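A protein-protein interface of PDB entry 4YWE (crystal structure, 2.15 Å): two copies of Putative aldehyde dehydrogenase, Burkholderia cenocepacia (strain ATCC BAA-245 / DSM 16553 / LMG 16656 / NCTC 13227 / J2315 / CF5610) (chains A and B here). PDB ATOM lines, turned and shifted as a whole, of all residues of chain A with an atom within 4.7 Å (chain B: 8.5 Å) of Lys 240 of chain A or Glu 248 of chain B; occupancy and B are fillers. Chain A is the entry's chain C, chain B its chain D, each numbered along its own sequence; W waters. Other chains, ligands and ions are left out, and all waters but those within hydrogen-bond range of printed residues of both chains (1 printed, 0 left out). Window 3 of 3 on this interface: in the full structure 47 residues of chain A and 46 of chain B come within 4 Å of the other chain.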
ATOM      1  N   PRO A 236     -18.382 -27.584   3.302  1.00  0.00           N
ATOM      2  CA  PRO A 236     -18.707 -27.052   1.974  1.00  0.00           C
ATOM      3  C   PRO A 236     -17.487 -26.935   1.063  1.00  0.00           C
ATOM      4  O   PRO A 236     -17.588 -27.210  -0.133  1.00  0.00           O
ATOM      5  CB  PRO A 236     -19.282 -25.668   2.285  1.00  0.00           C
ATOM      6  CG  PRO A 236     -19.837 -25.800   3.659  1.00  0.00           C
ATOM      7  CD  PRO A 236     -18.900 -26.722   4.380  1.00  0.00           C
ATOM      8  N   ALA A 237     -16.353 -26.531   1.628  1.00  0.00           N
ATOM      9  CA  ALA A 237     -15.125 -26.371   0.854  1.00  0.00           C
ATOM     10  C   ALA A 237     -14.663 -27.705   0.279  1.00  0.00           C
ATOM     11  O   ALA A 237     -14.338 -27.802  -0.904  1.00  0.00           O
ATOM     12  CB  ALA A 237     -14.031 -25.755   1.716  1.00  0.00           C
ATOM     13  N   THR A 238     -14.637 -28.730   1.124  1.00  0.00           N
ATOM     14  CA  THR A 238     -14.247 -30.067   0.695  1.00  0.00           C
ATOM     15  C   THR A 238     -15.308 -30.652  -0.233  1.00  0.00           C
ATOM     16  O   THR A 238     -14.988 -31.335  -1.205  1.00  0.00           O
ATOM     17  CB  THR A 238     -14.028 -31.006   1.899  1.00  0.00           C
ATOM     18  OG1 THR A 238     -12.968 -30.493   2.717  1.00  0.00           O
ATOM     19  CG2 THR A 238     -13.659 -32.407   1.432  1.00  0.00           C
ATOM     20  N   GLY A 239     -16.571 -30.367   0.065  1.00  0.00           N
ATOM     21  CA  GLY A 239     -17.673 -30.815  -0.770  1.00  0.00           C
ATOM     22  C   GLY A 239     -17.608 -30.250  -2.174  1.00  0.00           C
ATOM     23  O   GLY A 239     -18.041 -30.887  -3.135  1.00  0.00           O
ATOM     24  N   LYS A 240     -17.063 -29.044  -2.287  1.00  0.00           N
ATOM     25  CA  LYS A 240     -16.872 -28.399  -3.579  1.00  0.00           C
ATOM     26  C   LYS A 240     -15.789 -29.115  -4.379  1.00  0.00           C
ATOM     27  O   LYS A 240     -15.936 -29.335  -5.580  1.00  0.00           O
ATOM     28  CB  LYS A 240     -16.509 -26.927  -3.387  1.00  0.00           C
ATOM     29  CG  LYS A 240     -16.344 -26.148  -4.677  1.00  0.00           C
ATOM     30  CD  LYS A 240     -15.848 -24.741  -4.396  1.00  0.00           C
ATOM     31  CE  LYS A 240     -16.792 -24.001  -3.461  1.00  0.00           C
ATOM     32  NZ  LYS A 240     -16.299 -22.633  -3.137  1.00  0.00           N
ATOM     33  N   LEU A 241     -14.702 -29.479  -3.703  1.00  0.00           N
ATOM     34  CA  LEU A 241     -13.601 -30.193  -4.340  1.00  0.00           C
ATOM     35  C   LEU A 241     -14.039 -31.558  -4.853  1.00  0.00           C
ATOM     36  O   LEU A 241     -13.778 -31.907  -6.005  1.00  0.00           O
ATOM     37  CB  LEU A 241     -12.432 -30.361  -3.368  1.00  0.00           C
ATOM     38  CG  LEU A 241     -11.258 -29.395  -3.526  1.00  0.00           C
ATOM     39  CD1 LEU A 241     -10.117 -29.790  -2.601  1.00  0.00           C
ATOM     40  CD2 LEU A 241     -10.789 -29.353  -4.971  1.00  0.00           C
ATOM     41  N   VAL A 242     -14.697 -32.324  -3.987  1.00  0.00           N
ATOM     42  CA  VAL A 242     -15.153 -33.668  -4.322  1.00  0.00           C
ATOM     43  C   VAL A 242     -16.028 -33.648  -5.569  1.00  0.00           C
ATOM     44  O   VAL A 242     -15.875 -34.488  -6.457  1.00  0.00           O
ATOM     45  CB  VAL A 242     -15.908 -34.305  -3.142  1.00  0.00           C
ATOM     46  CG1 VAL A 242     -16.521 -35.637  -3.555  1.00  0.00           C
ATOM     47  CG2 VAL A 242     -14.978 -34.485  -1.955  1.00  0.00           C
ATOM     48  N   THR A 243     -16.937 -32.680  -5.629  1.00  0.00           N
ATOM     49  CA  THR A 243     -17.823 -32.520  -6.777  1.00  0.00           C
ATOM     50  C   THR A 243     -17.029 -32.273  -8.056  1.00  0.00           C
ATOM     51  O   THR A 243     -17.282 -32.895  -9.088  1.00  0.00           O
ATOM     52  CB  THR A 243     -18.814 -31.359  -6.563  1.00  0.00           C
ATOM     53  OG1 THR A 243     -19.682 -31.665  -5.465  1.00  0.00           O
ATOM     54  CG2 THR A 243     -19.649 -31.129  -7.815  1.00  0.00           C
ATOM     55  N   GLN A 244     -16.059 -31.368  -7.976  1.00  0.00           N
ATOM     56  CA  GLN A 244     -15.242 -31.016  -9.130  1.00  0.00           C
ATOM     57  C   GLN A 244     -14.286 -32.148  -9.500  1.00  0.00           C
ATOM     58  O   GLN A 244     -13.954 -32.331 -10.671  1.00  0.00           O
ATOM     59  CB  GLN A 244     -14.472 -29.723  -8.855  1.00  0.00           C
ATOM     60  CG  GLN A 244     -15.379 -28.512  -8.669  1.00  0.00           C
ATOM     61  CD  GLN A 244     -14.651 -27.299  -8.123  1.00  0.00           C
ATOM     62  OE1 GLN A 244     -13.572 -27.416  -7.546  1.00  0.00           O
ATOM     63  NE2 GLN A 244     -15.244 -26.125  -8.304  1.00  0.00           N
ATOM     64  N   ALA B 222     -23.983 -20.449 -15.421  1.00  0.00           N
ATOM     65  CA  ALA B 222     -23.538 -21.587 -14.620  1.00  0.00           C
ATOM     66  C   ALA B 222     -22.837 -21.146 -13.336  1.00  0.00           C
ATOM     67  O   ALA B 222     -22.747 -21.913 -12.376  1.00  0.00           O
ATOM     68  CB  ALA B 222     -22.618 -22.479 -15.441  1.00  0.00           C
ATOM     69  N   ARG B 223     -22.347 -19.911 -13.323  1.00  0.00           N
ATOM     70  CA  ARG B 223     -21.612 -19.383 -12.178  1.00  0.00           C
ATOM     71  C   ARG B 223     -22.502 -18.606 -11.212  1.00  0.00           C
ATOM     72  O   ARG B 223     -22.124 -18.379 -10.062  1.00  0.00           O
ATOM     73  CB  ARG B 223     -20.475 -18.472 -12.647  1.00  0.00           C
ATOM     74  CG  ARG B 223     -19.342 -19.179 -13.366  1.00  0.00           C
ATOM     75  CD  ARG B 223     -18.481 -18.168 -14.108  1.00  0.00           C
ATOM     76  NE  ARG B 223     -17.192 -18.721 -14.510  1.00  0.00           N
ATOM     77  CZ  ARG B 223     -16.358 -18.122 -15.353  1.00  0.00           C
ATOM     78  NH1 ARG B 223     -16.683 -16.953 -15.888  1.00  0.00           N
ATOM     79  NH2 ARG B 223     -15.202 -18.693 -15.664  1.00  0.00           N
ATOM     80  N   HIS B 224     -23.677 -18.194 -11.679  1.00  0.00           N
ATOM     81  CA  HIS B 224     -24.517 -17.281 -10.906  1.00  0.00           C
ATOM     82  C   HIS B 224     -25.065 -17.933  -9.638  1.00  0.00           C
ATOM     83  O   HIS B 224     -25.655 -19.013  -9.690  1.00  0.00           O
ATOM     84  CB  HIS B 224     -25.670 -16.756 -11.764  1.00  0.00           C
ATOM     85  CG  HIS B 224     -26.178 -15.417 -11.330  1.00  0.00           C
ATOM     86  ND1 HIS B 224     -27.131 -15.264 -10.346  1.00  0.00           N
ATOM     87  CD2 HIS B 224     -25.855 -14.167 -11.739  1.00  0.00           C
ATOM     88  CE1 HIS B 224     -27.378 -13.978 -10.171  1.00  0.00           C
ATOM     89  NE2 HIS B 224     -26.617 -13.290 -11.003  1.00  0.00           N
ATOM     90  N   PRO B 225     -24.862 -17.269  -8.489  1.00  0.00           N
ATOM     91  CA  PRO B 225     -25.313 -17.739  -7.173  1.00  0.00           C
ATOM     92  C   PRO B 225     -26.827 -17.676  -7.004  1.00  0.00           C
ATOM     93  O   PRO B 225     -27.364 -18.256  -6.059  1.00  0.00           O
ATOM     94  CB  PRO B 225     -24.625 -16.774  -6.198  1.00  0.00           C
ATOM     95  CG  PRO B 225     -23.530 -16.127  -6.985  1.00  0.00           C
ATOM     96  CD  PRO B 225     -24.051 -16.047  -8.380  1.00  0.00           C
ATOM     97  N   LEU B 241     -17.471 -28.720 -17.216  1.00  0.00           N
ATOM     98  CA  LEU B 241     -17.139 -27.358 -16.825  1.00  0.00           C
ATOM     99  C   LEU B 241     -18.298 -26.683 -16.094  1.00  0.00           C
ATOM    100  O   LEU B 241     -18.091 -25.998 -15.093  1.00  0.00           O
ATOM    101  CB  LEU B 241     -16.742 -26.538 -18.053  1.00  0.00           C
ATOM    102  CG  LEU B 241     -16.145 -25.157 -17.778  1.00  0.00           C
ATOM    103  CD1 LEU B 241     -14.884 -25.285 -16.940  1.00  0.00           C
ATOM    104  CD2 LEU B 241     -15.854 -24.428 -19.083  1.00  0.00           C
ATOM    105  N   VAL B 242     -19.512 -26.879 -16.598  1.00  0.00           N
ATOM    106  CA  VAL B 242     -20.702 -26.299 -15.982  1.00  0.00           C
ATOM    107  C   VAL B 242     -20.887 -26.845 -14.570  1.00  0.00           C
ATOM    108  O   VAL B 242     -21.186 -26.095 -13.638  1.00  0.00           O
ATOM    109  CB  VAL B 242     -21.955 -26.559 -16.840  1.00  0.00           C
ATOM    110  CG1 VAL B 242     -23.217 -26.186 -16.075  1.00  0.00           C
ATOM    111  CG2 VAL B 242     -21.872 -25.786 -18.148  1.00  0.00           C
ATOM    112  N   THR B 243     -20.699 -28.153 -14.420  1.00  0.00           N
ATOM    113  CA  THR B 243     -20.821 -28.811 -13.123  1.00  0.00           C
ATOM    114  C   THR B 243     -19.791 -28.264 -12.139  1.00  0.00           C
ATOM    115  O   THR B 243     -20.096 -28.021 -10.971  1.00  0.00           O
ATOM    116  CB  THR B 243     -20.643 -30.339 -13.246  1.00  0.00           C
ATOM    117  OG1 THR B 243     -21.668 -30.875 -14.092  1.00  0.00           O
ATOM    118  CG2 THR B 243     -20.724 -31.002 -11.880  1.00  0.00           C
ATOM    119  N   GLN B 244     -18.571 -28.065 -12.626  1.00  0.00           N
ATOM    120  CA  GLN B 244     -17.486 -27.560 -11.795  1.00  0.00           C
ATOM    121  C   GLN B 244     -17.701 -26.089 -11.451  1.00  0.00           C
ATOM    122  O   GLN B 244     -17.349 -25.645 -10.361  1.00  0.00           O
ATOM    123  CB  GLN B 244     -16.141 -27.765 -12.497  1.00  0.00           C
ATOM    124  CG  GLN B 244     -15.734 -29.228 -12.603  1.00  0.00           C
ATOM    125  CD  GLN B 244     -14.547 -29.451 -13.521  1.00  0.00           C
ATOM    126  OE1 GLN B 244     -14.127 -28.549 -14.245  1.00  0.00           O
ATOM    127  NE2 GLN B 244     -14.001 -30.661 -13.496  1.00  0.00           N
ATOM    128  N   MET B 245     -18.286 -25.341 -12.382  1.00  0.00           N
ATOM    129  CA  MET B 245     -18.609 -23.938 -12.141  1.00  0.00           C
ATOM    130  C   MET B 245     -19.743 -23.803 -11.134  1.00  0.00           C
ATOM    131  O   MET B 245     -19.690 -22.964 -10.232  1.00  0.00           O
ATOM    132  CB  MET B 245     -18.986 -23.235 -13.447  1.00  0.00           C
ATOM    133  CG  MET B 245     -17.806 -22.897 -14.341  1.00  0.00           C
ATOM    134  SD  MET B 245     -18.326 -22.278 -15.953  1.00  0.00           S
ATOM    135  CE  MET B 245     -16.771 -21.660 -16.590  1.00  0.00           C
ATOM    136  N   ALA B 246     -20.770 -24.634 -11.288  1.00  0.00           N
ATOM    137  CA  ALA B 246     -21.918 -24.599 -10.392  1.00  0.00           C
ATOM    138  C   ALA B 246     -21.560 -25.157  -9.018  1.00  0.00           C
ATOM    139  O   ALA B 246     -22.269 -24.922  -8.039  1.00  0.00           O
ATOM    140  CB  ALA B 246     -23.082 -25.371 -10.989  1.00  0.00           C
ATOM    141  N   ALA B 247     -20.455 -25.894  -8.951  1.00  0.00           N
ATOM    142  CA  ALA B 247     -19.986 -26.457  -7.690  1.00  0.00           C
ATOM    143  C   ALA B 247     -19.541 -25.353  -6.734  1.00  0.00           C
ATOM    144  O   ALA B 247     -19.505 -25.550  -5.521  1.00  0.00           O
ATOM    145  CB  ALA B 247     -18.852 -27.438  -7.933  1.00  0.00           C
ATOM    146  N   GLU B 248     -19.204 -24.194  -7.292  1.00  0.00           N
ATOM    147  CA  GLU B 248     -18.796 -23.042  -6.495  1.00  0.00           C
ATOM    148  C   GLU B 248     -19.958 -22.501  -5.670  1.00  0.00           C
ATOM    149  O   GLU B 248     -19.757 -21.870  -4.634  1.00  0.00           O
ATOM    150  CB  GLU B 248     -18.235 -21.938  -7.394  1.00  0.00           C
ATOM    151  CG  GLU B 248     -16.908 -22.286  -8.048  1.00  0.00           C
ATOM    152  CD  GLU B 248     -15.793 -22.478  -7.037  1.00  0.00           C
ATOM    153  OE1 GLU B 248     -15.824 -21.814  -5.979  1.00  0.00           O
ATOM    154  OE2 GLU B 248     -14.889 -23.300  -7.299  1.00  0.00           O
ATOM    155  N   ASN B 249     -21.177 -22.754  -6.137  1.00  0.00           N
ATOM    156  CA  ASN B 249     -22.373 -22.287  -5.450  1.00  0.00           C
ATOM    157  C   ASN B 249     -23.181 -23.461  -4.907  1.00  0.00           C
ATOM    158  O   ASN B 249     -24.308 -23.287  -4.440  1.00  0.00           O
ATOM    159  CB  ASN B 249     -23.232 -21.441  -6.393  1.00  0.00           C
ATOM    160  CG  ASN B 249     -22.508 -20.203  -6.887  1.00  0.00           C
ATOM    161  OD1 ASN B 249     -21.835 -19.516  -6.118  1.00  0.00           O
ATOM    162  ND2 ASN B 249     -22.637 -19.917  -8.176  1.00  0.00           N
ATOM    163  N   HIS B 250     -22.587 -24.651  -4.977  1.00  0.00           N
ATOM    164  CA  HIS B 250     -23.226 -25.892  -4.542  1.00  0.00           C
ATOM    165  C   HIS B 250     -24.565 -26.107  -5.244  1.00  0.00           C
ATOM    166  O   HIS B 250     -25.512 -26.636  -4.661  1.00  0.00           O
ATOM    167  CB  HIS B 250     -23.410 -25.896  -3.022  1.00  0.00           C
ATOM    168  CG  HIS B 250     -22.145 -25.635  -2.266  1.00  0.00           C
ATOM    169  ND1 HIS B 250     -21.161 -26.588  -2.113  1.00  0.00           N
ATOM    170  CD2 HIS B 250     -21.698 -24.527  -1.628  1.00  0.00           C
ATOM    171  CE1 HIS B 250     -20.164 -26.080  -1.409  1.00  0.00           C
ATOM    172  NE2 HIS B 250     -20.466 -24.830  -1.104  1.00  0.00           N
ATOM    173  N   VAL B 251     -24.626 -25.696  -6.506  1.00  0.00           N
ATOM    174  CA  VAL B 251     -25.832 -25.832  -7.308  1.00  0.00           C
ATOM    175  C   VAL B 251     -25.816 -27.159  -8.058  1.00  0.00           C
ATOM    176  O   VAL B 251     -24.861 -27.460  -8.778  1.00  0.00           O
ATOM    177  CB  VAL B 251     -25.983 -24.652  -8.286  1.00  0.00           C
ATOM    178  CG1 VAL B 251     -27.135 -24.895  -9.252  1.00  0.00           C
ATOM    179  CG2 VAL B 251     -26.180 -23.355  -7.521  1.00  0.00           C
HETATM  180  O   HOH W   1     -18.310 -21.443  -2.108  1.00  0.00           O
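The side-chain amino group (NZ) of Lys 240 of chain A is in salt-bridge range of the side-chain carboxylate (OE1) of Glu 248 of chain B (3.0 Å). The side-chain amide nitrogen (NE2) of Gln 244 of chain A is in hydrogen-bond range of the backbone carbonyl oxygen (O) of Gln 244 of chain B, at 3.0 Å. The side-chain amide nitrogen (NE2) of Gln 244 of chain A is in hydrogen-bond range of the side-chain carboxylate (OE2) of Glu 248 of chain B, 3.0 Å away.
The backbone carbonyl oxygen of Gly 239 of chain A lies within hydrogen-bond range of the side-chain hydroxyl of Thr 243 of chain A (3.0 Å).
Of the printed residues of chain B, Lys 240 of chain A touches Ala 247 (3.3 Å) and Glu 248 (3.0 Å). Of chain A, only Lys 240 and Gln 244 come within 4 Å of Glu 248 of chain B. No residue of chain B comes within 4 Å of Gly 239 of chain A. Printed residues of chain A within 4 Å of His 250 of chain B: Pro 236. Of the printed residues of chain A, Gln 244 of chain B touches Gln 244 (3.0 Å). Val 242 of chain A touches none of the printed residues of chain B. Asn 249 of chain B touches none of the printed residues of chain A. The nearest residue of chain B that does not touch Lys 240 of chain A is His 250 of chain B (4.2 Å). The nearest printed residue of chain A that does not touch Glu 248 of chain B is Thr 243 of chain A (7.0 Å). The nearest printed residue of chain B that does not touch Pro 236 of chain A is Ala 247 of chain B (6.0 Å).
Printed residues of chain A that touch a printed residue of chain B: Pro 236, Lys 240, Thr 243 and Gln 244. Hydrophobic or aromatic side chains of chain A within 4 Å of the printed part of chain B: Pro 236. Hydrophobic or aromatic side chains of chain B within 4 Å of the printed part of chain A: Ala 247 and His 250. Among the printed residues, 7 pairs touch across the chains.
Water W1 lies within hydrogen-bond range of the side-chain amino group (NZ) of Lys 240 of chain A (2.6 Å) and the backbone carbonyl oxygen (O) of Glu 248 of chain B (2.9 Å).
Among the printed residues, merely in contact across the chains: Pro 236 of chain A with His 250 of chain B (3.1 Å), Lys 240 of chain A with Ala 247 of chain B (3.3 Å), Gln 244 of chain A with Ala 247 of chain B (3.7 Å) and Thr 243 of chain A with Ala 247 of chain B (3.8 Å).
Gln 244 of chain A touches its own counterpart, Gln 244 of chain B. Positions printed for both chains: 241, 242, 243 and 244. Of the 7 pairs that touch across the chains among the printed residues, 1 has its exchanged pair printed and touching as well.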
